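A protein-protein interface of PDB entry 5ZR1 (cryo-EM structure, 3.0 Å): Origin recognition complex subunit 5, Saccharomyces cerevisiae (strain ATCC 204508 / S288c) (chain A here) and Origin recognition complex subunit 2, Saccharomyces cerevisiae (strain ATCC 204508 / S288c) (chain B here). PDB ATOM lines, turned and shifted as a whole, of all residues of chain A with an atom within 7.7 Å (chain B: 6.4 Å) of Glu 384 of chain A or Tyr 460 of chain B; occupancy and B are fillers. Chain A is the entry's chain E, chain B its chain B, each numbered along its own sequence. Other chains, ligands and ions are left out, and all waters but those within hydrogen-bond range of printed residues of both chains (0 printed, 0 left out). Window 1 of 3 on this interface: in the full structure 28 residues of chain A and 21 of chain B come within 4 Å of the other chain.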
ATOM      1  N   CYS A 338       5.495  -1.120 -36.480  1.00  0.00           N
ATOM      2  CA  CYS A 338       6.762  -0.866 -35.795  1.00  0.00           C
ATOM      3  C   CYS A 338       7.908  -1.665 -36.387  1.00  0.00           C
ATOM      4  O   CYS A 338       9.067  -1.252 -36.293  1.00  0.00           O
ATOM      5  CB  CYS A 338       6.653  -1.210 -34.313  1.00  0.00           C
ATOM      6  SG  CYS A 338       5.620  -0.154 -33.327  1.00  0.00           S
ATOM      7  N   PHE A 381      11.859  -4.076 -32.477  1.00  0.00           N
ATOM      8  CA  PHE A 381      11.427  -2.819 -31.890  1.00  0.00           C
ATOM      9  C   PHE A 381      11.351  -2.952 -30.377  1.00  0.00           C
ATOM     10  O   PHE A 381      11.439  -4.045 -29.817  1.00  0.00           O
ATOM     11  CB  PHE A 381      10.081  -2.344 -32.470  1.00  0.00           C
ATOM     12  CG  PHE A 381       8.951  -3.342 -32.357  1.00  0.00           C
ATOM     13  CD1 PHE A 381       8.667  -4.192 -33.404  1.00  0.00           C
ATOM     14  CD2 PHE A 381       8.148  -3.401 -31.231  1.00  0.00           C
ATOM     15  CE1 PHE A 381       7.627  -5.091 -33.323  1.00  0.00           C
ATOM     16  CE2 PHE A 381       7.118  -4.310 -31.144  1.00  0.00           C
ATOM     17  CZ  PHE A 381       6.855  -5.149 -32.192  1.00  0.00           C
ATOM     18  N   ALA A 382      11.184  -1.813 -29.719  1.00  0.00           N
ATOM     19  CA  ALA A 382      11.052  -1.761 -28.273  1.00  0.00           C
ATOM     20  C   ALA A 382       9.584  -1.783 -27.876  1.00  0.00           C
ATOM     21  O   ALA A 382       8.691  -1.554 -28.692  1.00  0.00           O
ATOM     22  CB  ALA A 382      11.725  -0.511 -27.712  1.00  0.00           C
ATOM     23  N   ILE A 383       9.343  -2.049 -26.591  1.00  0.00           N
ATOM     24  CA  ILE A 383       7.980  -2.225 -26.111  1.00  0.00           C
ATOM     25  C   ILE A 383       7.237  -0.896 -26.014  1.00  0.00           C
ATOM     26  O   ILE A 383       6.006  -0.871 -26.101  1.00  0.00           O
ATOM     27  CB  ILE A 383       8.004  -2.988 -24.767  1.00  0.00           C
ATOM     28  CG1 ILE A 383       6.617  -3.511 -24.391  1.00  0.00           C
ATOM     29  CG2 ILE A 383       8.599  -2.140 -23.649  1.00  0.00           C
ATOM     30  CD1 ILE A 383       6.106  -4.561 -25.330  1.00  0.00           C
ATOM     31  N   GLU A 384       7.949   0.225 -25.898  1.00  0.00           N
ATOM     32  CA  GLU A 384       7.264   1.500 -25.725  1.00  0.00           C
ATOM     33  C   GLU A 384       6.846   2.098 -27.061  1.00  0.00           C
ATOM     34  O   GLU A 384       5.836   2.807 -27.127  1.00  0.00           O
ATOM     35  CB  GLU A 384       8.156   2.471 -24.948  1.00  0.00           C
ATOM     36  CG  GLU A 384       7.469   3.757 -24.503  1.00  0.00           C
ATOM     37  CD  GLU A 384       6.409   3.535 -23.435  1.00  0.00           C
ATOM     38  OE1 GLU A 384       6.504   2.552 -22.680  1.00  0.00           O
ATOM     39  OE2 GLU A 384       5.477   4.355 -23.346  1.00  0.00           O
ATOM     40  N   ARG A 385       7.605   1.825 -28.126  1.00  0.00           N
ATOM     41  CA  ARG A 385       7.203   2.246 -29.464  1.00  0.00           C
ATOM     42  C   ARG A 385       5.929   1.539 -29.903  1.00  0.00           C
ATOM     43  O   ARG A 385       5.091   2.129 -30.594  1.00  0.00           O
ATOM     44  CB  ARG A 385       8.321   1.958 -30.464  1.00  0.00           C
ATOM     45  CG  ARG A 385       8.041   2.499 -31.844  1.00  0.00           C
ATOM     46  CD  ARG A 385       8.994   1.977 -32.878  1.00  0.00           C
ATOM     47  NE  ARG A 385       8.577   2.423 -34.200  1.00  0.00           N
ATOM     48  CZ  ARG A 385       9.091   1.970 -35.335  1.00  0.00           C
ATOM     49  NH1 ARG A 385      10.024   1.034 -35.305  1.00  0.00           N
ATOM     50  NH2 ARG A 385       8.645   2.430 -36.493  1.00  0.00           N
ATOM     51  N   LEU A 386       5.776   0.272 -29.512  1.00  0.00           N
ATOM     52  CA  LEU A 386       4.563  -0.476 -29.817  1.00  0.00           C
ATOM     53  C   LEU A 386       3.346   0.139 -29.148  1.00  0.00           C
ATOM     54  O   LEU A 386       2.291   0.274 -29.772  1.00  0.00           O
ATOM     55  CB  LEU A 386       4.727  -1.929 -29.385  1.00  0.00           C
ATOM     56  CG  LEU A 386       3.517  -2.834 -29.572  1.00  0.00           C
ATOM     57  CD1 LEU A 386       3.126  -2.875 -31.017  1.00  0.00           C
ATOM     58  CD2 LEU A 386       3.838  -4.221 -29.074  1.00  0.00           C
ATOM     59  N   LEU A 387       3.480   0.543 -27.887  1.00  0.00           N
ATOM     60  CA  LEU A 387       2.363   1.136 -27.170  1.00  0.00           C
ATOM     61  C   LEU A 387       2.090   2.565 -27.613  1.00  0.00           C
ATOM     62  O   LEU A 387       0.991   3.074 -27.377  1.00  0.00           O
ATOM     63  CB  LEU A 387       2.643   1.095 -25.675  1.00  0.00           C
ATOM     64  CG  LEU A 387       2.861  -0.280 -25.055  1.00  0.00           C
ATOM     65  CD1 LEU A 387       3.276  -0.112 -23.613  1.00  0.00           C
ATOM     66  CD2 LEU A 387       1.619  -1.135 -25.166  1.00  0.00           C
ATOM     67  N   ALA A 388       3.062   3.224 -28.243  1.00  0.00           N
ATOM     68  CA  ALA A 388       2.820   4.547 -28.802  1.00  0.00           C
ATOM     69  C   ALA A 388       2.049   4.455 -30.111  1.00  0.00           C
ATOM     70  O   ALA A 388       1.082   5.190 -30.322  1.00  0.00           O
ATOM     71  CB  ALA A 388       4.141   5.279 -29.013  1.00  0.00           C
ATOM     72  N   ILE A 389       2.454   3.547 -30.997  1.00  0.00           N
ATOM     73  CA  ILE A 389       1.741   3.366 -32.252  1.00  0.00           C
ATOM     74  C   ILE A 389       0.404   2.658 -32.032  1.00  0.00           C
ATOM     75  O   ILE A 389      -0.527   2.848 -32.822  1.00  0.00           O
ATOM     76  CB  ILE A 389       2.709   2.682 -33.246  1.00  0.00           C
ATOM     77  CG1 ILE A 389       3.801   3.686 -33.613  1.00  0.00           C
ATOM     78  CG2 ILE A 389       2.045   2.184 -34.518  1.00  0.00           C
ATOM     79  CD1 ILE A 389       4.882   3.165 -34.494  1.00  0.00           C
ATOM     80  N   PHE A 390       0.251   1.926 -30.924  1.00  0.00           N
ATOM     81  CA  PHE A 390      -1.041   1.326 -30.589  1.00  0.00           C
ATOM     82  C   PHE A 390      -2.102   2.383 -30.313  1.00  0.00           C
ATOM     83  O   PHE A 390      -3.199   2.327 -30.873  1.00  0.00           O
ATOM     84  CB  PHE A 390      -0.908   0.391 -29.389  1.00  0.00           C
ATOM     85  CG  PHE A 390      -2.217  -0.126 -28.879  1.00  0.00           C
ATOM     86  CD1 PHE A 390      -2.936  -1.059 -29.601  1.00  0.00           C
ATOM     87  CD2 PHE A 390      -2.719   0.311 -27.665  1.00  0.00           C
ATOM     88  CE1 PHE A 390      -4.141  -1.529 -29.127  1.00  0.00           C
ATOM     89  CE2 PHE A 390      -3.919  -0.158 -27.189  1.00  0.00           C
ATOM     90  CZ  PHE A 390      -4.630  -1.079 -27.920  1.00  0.00           C
ATOM     91  N   GLN A 391      -1.798   3.363 -29.465  1.00  0.00           N
ATOM     92  CA  GLN A 391      -2.816   4.374 -29.219  1.00  0.00           C
ATOM     93  C   GLN A 391      -2.858   5.445 -30.296  1.00  0.00           C
ATOM     94  O   GLN A 391      -3.767   6.277 -30.279  1.00  0.00           O
ATOM     95  CB  GLN A 391      -2.637   5.032 -27.853  1.00  0.00           C
ATOM     96  CG  GLN A 391      -1.405   5.864 -27.698  1.00  0.00           C
ATOM     97  CD  GLN A 391      -1.415   6.640 -26.401  1.00  0.00           C
ATOM     98  OE1 GLN A 391      -2.397   6.636 -25.668  1.00  0.00           O
ATOM     99  NE2 GLN A 391      -0.324   7.321 -26.118  1.00  0.00           N
ATOM    100  N   ALA A 416      -2.808   2.306 -21.608  1.00  0.00           N
ATOM    101  CA  ALA A 416      -2.479   0.885 -21.516  1.00  0.00           C
ATOM    102  C   ALA A 416      -2.917   0.369 -20.153  1.00  0.00           C
ATOM    103  O   ALA A 416      -2.184   0.452 -19.168  1.00  0.00           O
ATOM    104  CB  ALA A 416      -0.991   0.659 -21.739  1.00  0.00           C
ATOM    105  N   PHE A 421      -1.574  -5.199 -21.769  1.00  0.00           N
ATOM    106  CA  PHE A 421      -0.427  -6.045 -21.467  1.00  0.00           C
ATOM    107  C   PHE A 421      -0.794  -7.517 -21.383  1.00  0.00           C
ATOM    108  O   PHE A 421       0.046  -8.372 -21.673  1.00  0.00           O
ATOM    109  CB  PHE A 421       0.216  -5.608 -20.159  1.00  0.00           C
ATOM    110  CG  PHE A 421       0.954  -4.320 -20.255  1.00  0.00           C
ATOM    111  CD1 PHE A 421       2.215  -4.281 -20.819  1.00  0.00           C
ATOM    112  CD2 PHE A 421       0.399  -3.150 -19.777  1.00  0.00           C
ATOM    113  CE1 PHE A 421       2.904  -3.101 -20.912  1.00  0.00           C
ATOM    114  CE2 PHE A 421       1.087  -1.964 -19.867  1.00  0.00           C
ATOM    115  CZ  PHE A 421       2.341  -1.941 -20.436  1.00  0.00           C
ATOM    116  N   TYR A 443      10.717 -10.768 -19.968  1.00  0.00           N
ATOM    117  CA  TYR A 443       9.897  -9.698 -20.524  1.00  0.00           C
ATOM    118  C   TYR A 443      10.281  -8.349 -19.939  1.00  0.00           C
ATOM    119  O   TYR A 443      10.213  -7.323 -20.624  1.00  0.00           O
ATOM    120  CB  TYR A 443       8.429  -9.958 -20.198  1.00  0.00           C
ATOM    121  CG  TYR A 443       7.836 -11.246 -20.709  1.00  0.00           C
ATOM    122  CD1 TYR A 443       7.253 -11.318 -21.964  1.00  0.00           C
ATOM    123  CD2 TYR A 443       7.850 -12.390 -19.926  1.00  0.00           C
ATOM    124  CE1 TYR A 443       6.696 -12.498 -22.428  1.00  0.00           C
ATOM    125  CE2 TYR A 443       7.302 -13.573 -20.380  1.00  0.00           C
ATOM    126  CZ  TYR A 443       6.727 -13.621 -21.629  1.00  0.00           C
ATOM    127  OH  TYR A 443       6.183 -14.801 -22.075  1.00  0.00           O
ATOM    128  N   LEU A 444      10.690  -8.346 -18.676  1.00  0.00           N
ATOM    129  CA  LEU A 444      10.793  -7.170 -17.823  1.00  0.00           C
ATOM    130  C   LEU A 444      12.196  -6.583 -17.852  1.00  0.00           C
ATOM    131  O   LEU A 444      12.782  -6.295 -16.813  1.00  0.00           O
ATOM    132  CB  LEU A 444      10.411  -7.564 -16.402  1.00  0.00           C
ATOM    133  CG  LEU A 444       8.976  -7.707 -15.899  1.00  0.00           C
ATOM    134  CD1 LEU A 444       8.344  -6.400 -15.993  1.00  0.00           C
ATOM    135  CD2 LEU A 444       8.137  -8.711 -16.647  1.00  0.00           C
ATOM    136  N   SER A 445      12.750  -6.383 -19.039  1.00  0.00           N
ATOM    137  CA  SER A 445      14.144  -5.996 -19.131  1.00  0.00           C
ATOM    138  C   SER A 445      14.322  -4.954 -20.219  1.00  0.00           C
ATOM    139  O   SER A 445      13.541  -4.907 -21.176  1.00  0.00           O
ATOM    140  CB  SER A 445      15.046  -7.204 -19.419  1.00  0.00           C
ATOM    141  OG  SER A 445      14.756  -7.742 -20.684  1.00  0.00           O
ATOM    142  N   PRO A 446      15.325  -4.087 -20.080  1.00  0.00           N
ATOM    143  CA  PRO A 446      15.562  -3.078 -21.116  1.00  0.00           C
ATOM    144  C   PRO A 446      16.069  -3.651 -22.422  1.00  0.00           C
ATOM    145  O   PRO A 446      15.816  -3.069 -23.483  1.00  0.00           O
ATOM    146  CB  PRO A 446      16.619  -2.184 -20.469  1.00  0.00           C
ATOM    147  CG  PRO A 446      16.453  -2.366 -19.028  1.00  0.00           C
ATOM    148  CD  PRO A 446      16.102  -3.798 -18.862  1.00  0.00           C
ATOM    149  N   TRP A 450      11.385  -6.848 -29.561  1.00  0.00           N
ATOM    150  CA  TRP A 450      10.223  -7.583 -30.012  1.00  0.00           C
ATOM    151  C   TRP A 450      10.110  -7.441 -31.518  1.00  0.00           C
ATOM    152  O   TRP A 450      10.587  -6.470 -32.103  1.00  0.00           O
ATOM    153  CB  TRP A 450       8.970  -7.038 -29.329  1.00  0.00           C
ATOM    154  CG  TRP A 450       8.996  -7.201 -27.850  1.00  0.00           C
ATOM    155  CD1 TRP A 450       9.583  -6.367 -26.948  1.00  0.00           C
ATOM    156  CD2 TRP A 450       8.361  -8.228 -27.089  1.00  0.00           C
ATOM    157  NE1 TRP A 450       9.388  -6.836 -25.673  1.00  0.00           N
ATOM    158  CE2 TRP A 450       8.635  -7.975 -25.735  1.00  0.00           C
ATOM    159  CE3 TRP A 450       7.601  -9.346 -27.422  1.00  0.00           C
ATOM    160  CZ2 TRP A 450       8.172  -8.797 -24.720  1.00  0.00           C
ATOM    161  CZ3 TRP A 450       7.143 -10.153 -26.419  1.00  0.00           C
ATOM    162  CH2 TRP A 450       7.426  -9.879 -25.084  1.00  0.00           C
ATOM    163  N   TYR B 246       6.043  10.874 -27.117  1.00  0.00           N
ATOM    164  CA  TYR B 246       7.027   9.860 -27.479  1.00  0.00           C
ATOM    165  C   TYR B 246       7.710  10.213 -28.791  1.00  0.00           C
ATOM    166  O   TYR B 246       8.936  10.129 -28.909  1.00  0.00           O
ATOM    167  CB  TYR B 246       6.350   8.495 -27.585  1.00  0.00           C
ATOM    168  CG  TYR B 246       7.291   7.351 -27.885  1.00  0.00           C
ATOM    169  CD1 TYR B 246       8.044   6.780 -26.882  1.00  0.00           C
ATOM    170  CD2 TYR B 246       7.430   6.849 -29.170  1.00  0.00           C
ATOM    171  CE1 TYR B 246       8.909   5.742 -27.139  1.00  0.00           C
ATOM    172  CE2 TYR B 246       8.294   5.812 -29.438  1.00  0.00           C
ATOM    173  CZ  TYR B 246       9.024   5.260 -28.417  1.00  0.00           C
ATOM    174  OH  TYR B 246       9.894   4.227 -28.664  1.00  0.00           O
ATOM    175  N   ASP B 428       7.702  -9.543  -9.510  1.00  0.00           N
ATOM    176  CA  ASP B 428       8.438  -9.261 -10.734  1.00  0.00           C
ATOM    177  C   ASP B 428       9.922  -9.003 -10.482  1.00  0.00           C
ATOM    178  O   ASP B 428      10.572  -8.306 -11.267  1.00  0.00           O
ATOM    179  CB  ASP B 428       7.798  -8.076 -11.447  1.00  0.00           C
ATOM    180  CG  ASP B 428       7.646  -6.870 -10.546  1.00  0.00           C
ATOM    181  OD1 ASP B 428       7.980  -6.946  -9.347  1.00  0.00           O
ATOM    182  OD2 ASP B 428       7.169  -5.835 -11.039  1.00  0.00           O
ATOM    183  N   ASP B 457       6.956  -4.228  -8.396  1.00  0.00           N
ATOM    184  CA  ASP B 457       7.548  -2.902  -8.545  1.00  0.00           C
ATOM    185  C   ASP B 457       7.720  -2.434  -9.979  1.00  0.00           C
ATOM    186  O   ASP B 457       7.633  -1.230 -10.219  1.00  0.00           O
ATOM    187  CB  ASP B 457       8.921  -2.826  -7.864  1.00  0.00           C
ATOM    188  CG  ASP B 457       8.827  -2.577  -6.377  1.00  0.00           C
ATOM    189  OD1 ASP B 457       7.816  -1.998  -5.930  1.00  0.00           O
ATOM    190  OD2 ASP B 457       9.789  -2.913  -5.658  1.00  0.00           O
ATOM    191  N   HIS B 458       7.988  -3.328 -10.927  1.00  0.00           N
ATOM    192  CA  HIS B 458       8.305  -2.897 -12.282  1.00  0.00           C
ATOM    193  C   HIS B 458       7.046  -2.384 -12.968  1.00  0.00           C
ATOM    194  O   HIS B 458       5.934  -2.834 -12.690  1.00  0.00           O
ATOM    195  CB  HIS B 458       8.913  -4.047 -13.085  1.00  0.00           C
ATOM    196  CG  HIS B 458       9.676  -3.610 -14.294  1.00  0.00           C
ATOM    197  ND1 HIS B 458       9.065  -3.197 -15.454  1.00  0.00           N
ATOM    198  CD2 HIS B 458      11.005  -3.585 -14.543  1.00  0.00           C
ATOM    199  CE1 HIS B 458       9.981  -2.893 -16.352  1.00  0.00           C
ATOM    200  NE2 HIS B 458      11.168  -3.128 -15.827  1.00  0.00           N
ATOM    201  N   ILE B 459       7.228  -1.415 -13.862  1.00  0.00           N
ATOM    202  CA  ILE B 459       6.079  -0.739 -14.448  1.00  0.00           C
ATOM    203  C   ILE B 459       5.468  -1.544 -15.596  1.00  0.00           C
ATOM    204  O   ILE B 459       4.281  -1.370 -15.901  1.00  0.00           O
ATOM    205  CB  ILE B 459       6.498   0.690 -14.846  1.00  0.00           C
ATOM    206  CG1 ILE B 459       5.276   1.575 -15.088  1.00  0.00           C
ATOM    207  CG2 ILE B 459       7.420   0.677 -16.042  1.00  0.00           C
ATOM    208  CD1 ILE B 459       5.568   3.042 -15.131  1.00  0.00           C
ATOM    209  N   TYR B 460       6.216  -2.460 -16.210  1.00  0.00           N
ATOM    210  CA  TYR B 460       5.656  -3.373 -17.197  1.00  0.00           C
ATOM    211  C   TYR B 460       5.372  -4.748 -16.619  1.00  0.00           C
ATOM    212  O   TYR B 460       5.405  -5.733 -17.356  1.00  0.00           O
ATOM    213  CB  TYR B 460       6.581  -3.531 -18.404  1.00  0.00           C
ATOM    214  CG  TYR B 460       6.850  -2.260 -19.149  1.00  0.00           C
ATOM    215  CD1 TYR B 460       5.843  -1.617 -19.843  1.00  0.00           C
ATOM    216  CD2 TYR B 460       8.129  -1.738 -19.215  1.00  0.00           C
ATOM    217  CE1 TYR B 460       6.086  -0.461 -20.538  1.00  0.00           C
ATOM    218  CE2 TYR B 460       8.387  -0.585 -19.912  1.00  0.00           C
ATOM    219  CZ  TYR B 460       7.361   0.047 -20.571  1.00  0.00           C
ATOM    220  OH  TYR B 460       7.620   1.196 -21.268  1.00  0.00           O
ATOM    221  N   ALA B 461       5.157  -4.843 -15.316  1.00  0.00           N
ATOM    222  CA  ALA B 461       4.760  -6.087 -14.657  1.00  0.00           C
ATOM    223  C   ALA B 461       3.524  -6.812 -15.212  1.00  0.00           C
ATOM    224  O   ALA B 461       3.530  -8.047 -15.187  1.00  0.00           O
ATOM    225  CB  ALA B 461       4.559  -5.832 -13.162  1.00  0.00           C
ATOM    226  N   PRO B 462       2.458  -6.158 -15.715  1.00  0.00           N
ATOM    227  CA  PRO B 462       1.348  -6.946 -16.280  1.00  0.00           C
ATOM    228  C   PRO B 462       1.653  -7.612 -17.608  1.00  0.00           C
ATOM    229  O   PRO B 462       0.823  -8.396 -18.082  1.00  0.00           O
ATOM    230  CB  PRO B 462       0.232  -5.915 -16.442  1.00  0.00           C
ATOM    231  CG  PRO B 462       0.578  -4.854 -15.551  1.00  0.00           C
ATOM    232  CD  PRO B 462       2.019  -4.756 -15.572  1.00  0.00           C
ATOM    233  N   LEU B 463       2.808  -7.341 -18.219  1.00  0.00           N
ATOM    234  CA  LEU B 463       3.258  -8.035 -19.420  1.00  0.00           C
ATOM    235  C   LEU B 463       3.679  -9.467 -19.127  1.00  0.00           C
ATOM    236  O   LEU B 463       3.883 -10.256 -20.053  1.00  0.00           O
ATOM    237  CB  LEU B 463       4.420  -7.249 -20.039  1.00  0.00           C
ATOM    238  CG  LEU B 463       5.030  -7.555 -21.402  1.00  0.00           C
ATOM    239  CD1 LEU B 463       3.985  -7.344 -22.455  1.00  0.00           C
ATOM    240  CD2 LEU B 463       6.236  -6.680 -21.661  1.00  0.00           C
ATOM    241  N   LEU B 464       3.787  -9.819 -17.857  1.00  0.00           N
ATOM    242  CA  LEU B 464       4.328 -11.083 -17.408  1.00  0.00           C
ATOM    243  C   LEU B 464       3.267 -12.166 -17.275  1.00  0.00           C
ATOM    244  O   LEU B 464       3.616 -13.331 -17.059  1.00  0.00           O
ATOM    245  CB  LEU B 464       5.050 -10.829 -16.082  1.00  0.00           C
ATOM    246  CG  LEU B 464       5.962 -11.821 -15.394  1.00  0.00           C
ATOM    247  CD1 LEU B 464       7.036 -12.236 -16.361  1.00  0.00           C
ATOM    248  CD2 LEU B 464       6.571 -11.124 -14.207  1.00  0.00           C
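Of the printed residues of chain B, Ala 388 of chain A touches Tyr 246. Gln 391 of chain A touches none of the printed residues of chain B. Of the printed residues of chain B, Phe 421 of chain A touches Tyr 460 (3.5 Å), Pro 462 (3.5 Å) and Leu 463 (3.7 Å). Printed residues of chain A within 4 Å of Tyr 246 of chain B: Glu 384 (3.6 Å), Arg 385 (3.3 Å) and Ala 388 (3.6 Å). Tyr 460 of chain B touches four residues of chain A. Printed residues of chain A within 4 Å of Ala 461 of chain B: Leu 444. Of the printed residues of chain A, Pro 462 of chain B touches Phe 421 (3.5 Å). The nearest residue of chain A that does not touch Tyr 460 of chain B is Leu 387 of chain A (4.2 Å).
Among the printed residues, pairs that only touch across the chains: Ile 383 of chain A with Tyr 460 of chain B (3.97 Å), Glu 384 of chain A with Tyr 246 of chain B (3.6 Å), Ala 388 of chain A with Tyr 246 of chain B (3.6 Å), Phe 421 of chain A with Tyr 460 of chain B (3.5 Å), Phe 421 of chain A with Pro 462 of chain B (3.5 Å), Phe 421 of chain A with Leu 463 of chain B (3.7 Å), Tyr 443 of chain A with Leu 464 of chain B (3.7 Å), Leu 444 of chain A with His 458 of chain B (3.3 Å), Leu 444 of chain A with Tyr 460 of chain B (3.3 Å), Leu 444 of chain A with Ala 461 of chain B (3.6 Å) and Leu 444 of chain A with Leu 464 of chain B (3.7 Å).
ND1 of His 458 of chain B is in hydrogen-bond range of N of Tyr 460 of chain B (3.0 Å). N of His 458 of chain B sits at hydrogen-bond distance from OD2 of Asp 428 of chain B (2.6 Å). The guanidinium group of Arg 385 of chain A sits at hydrogen-bond distance from the backbone carbonyl oxygen of Cys 338 of chain A.
Of the 10 printed residues of chain B, 7 touch a printed residue of chain A. Hydrophobic or aromatic side chains of chain B that line the printed part of chain A: Tyr 246, His 458, Tyr 460, Pro 462, Leu 463 and Leu 464. Of the 19 printed residues of chain A, 7 touch a printed residue of chain B. Hydrophobic or aromatic side chains of chain A that line the printed part of chain B: Ile 383, Ala 388, Phe 421, Tyr 443 and Leu 444.
The side-chain carboxylate of Glu 384 of chain A sits close to the side-chain hydroxyl of Tyr 460 of chain B (2.3 Å). The side-chain hydroxyl (OH) of Tyr 246 of chain B sits close to the backbone NH (N) of Arg 385 of chain A, 3.4 Å away.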
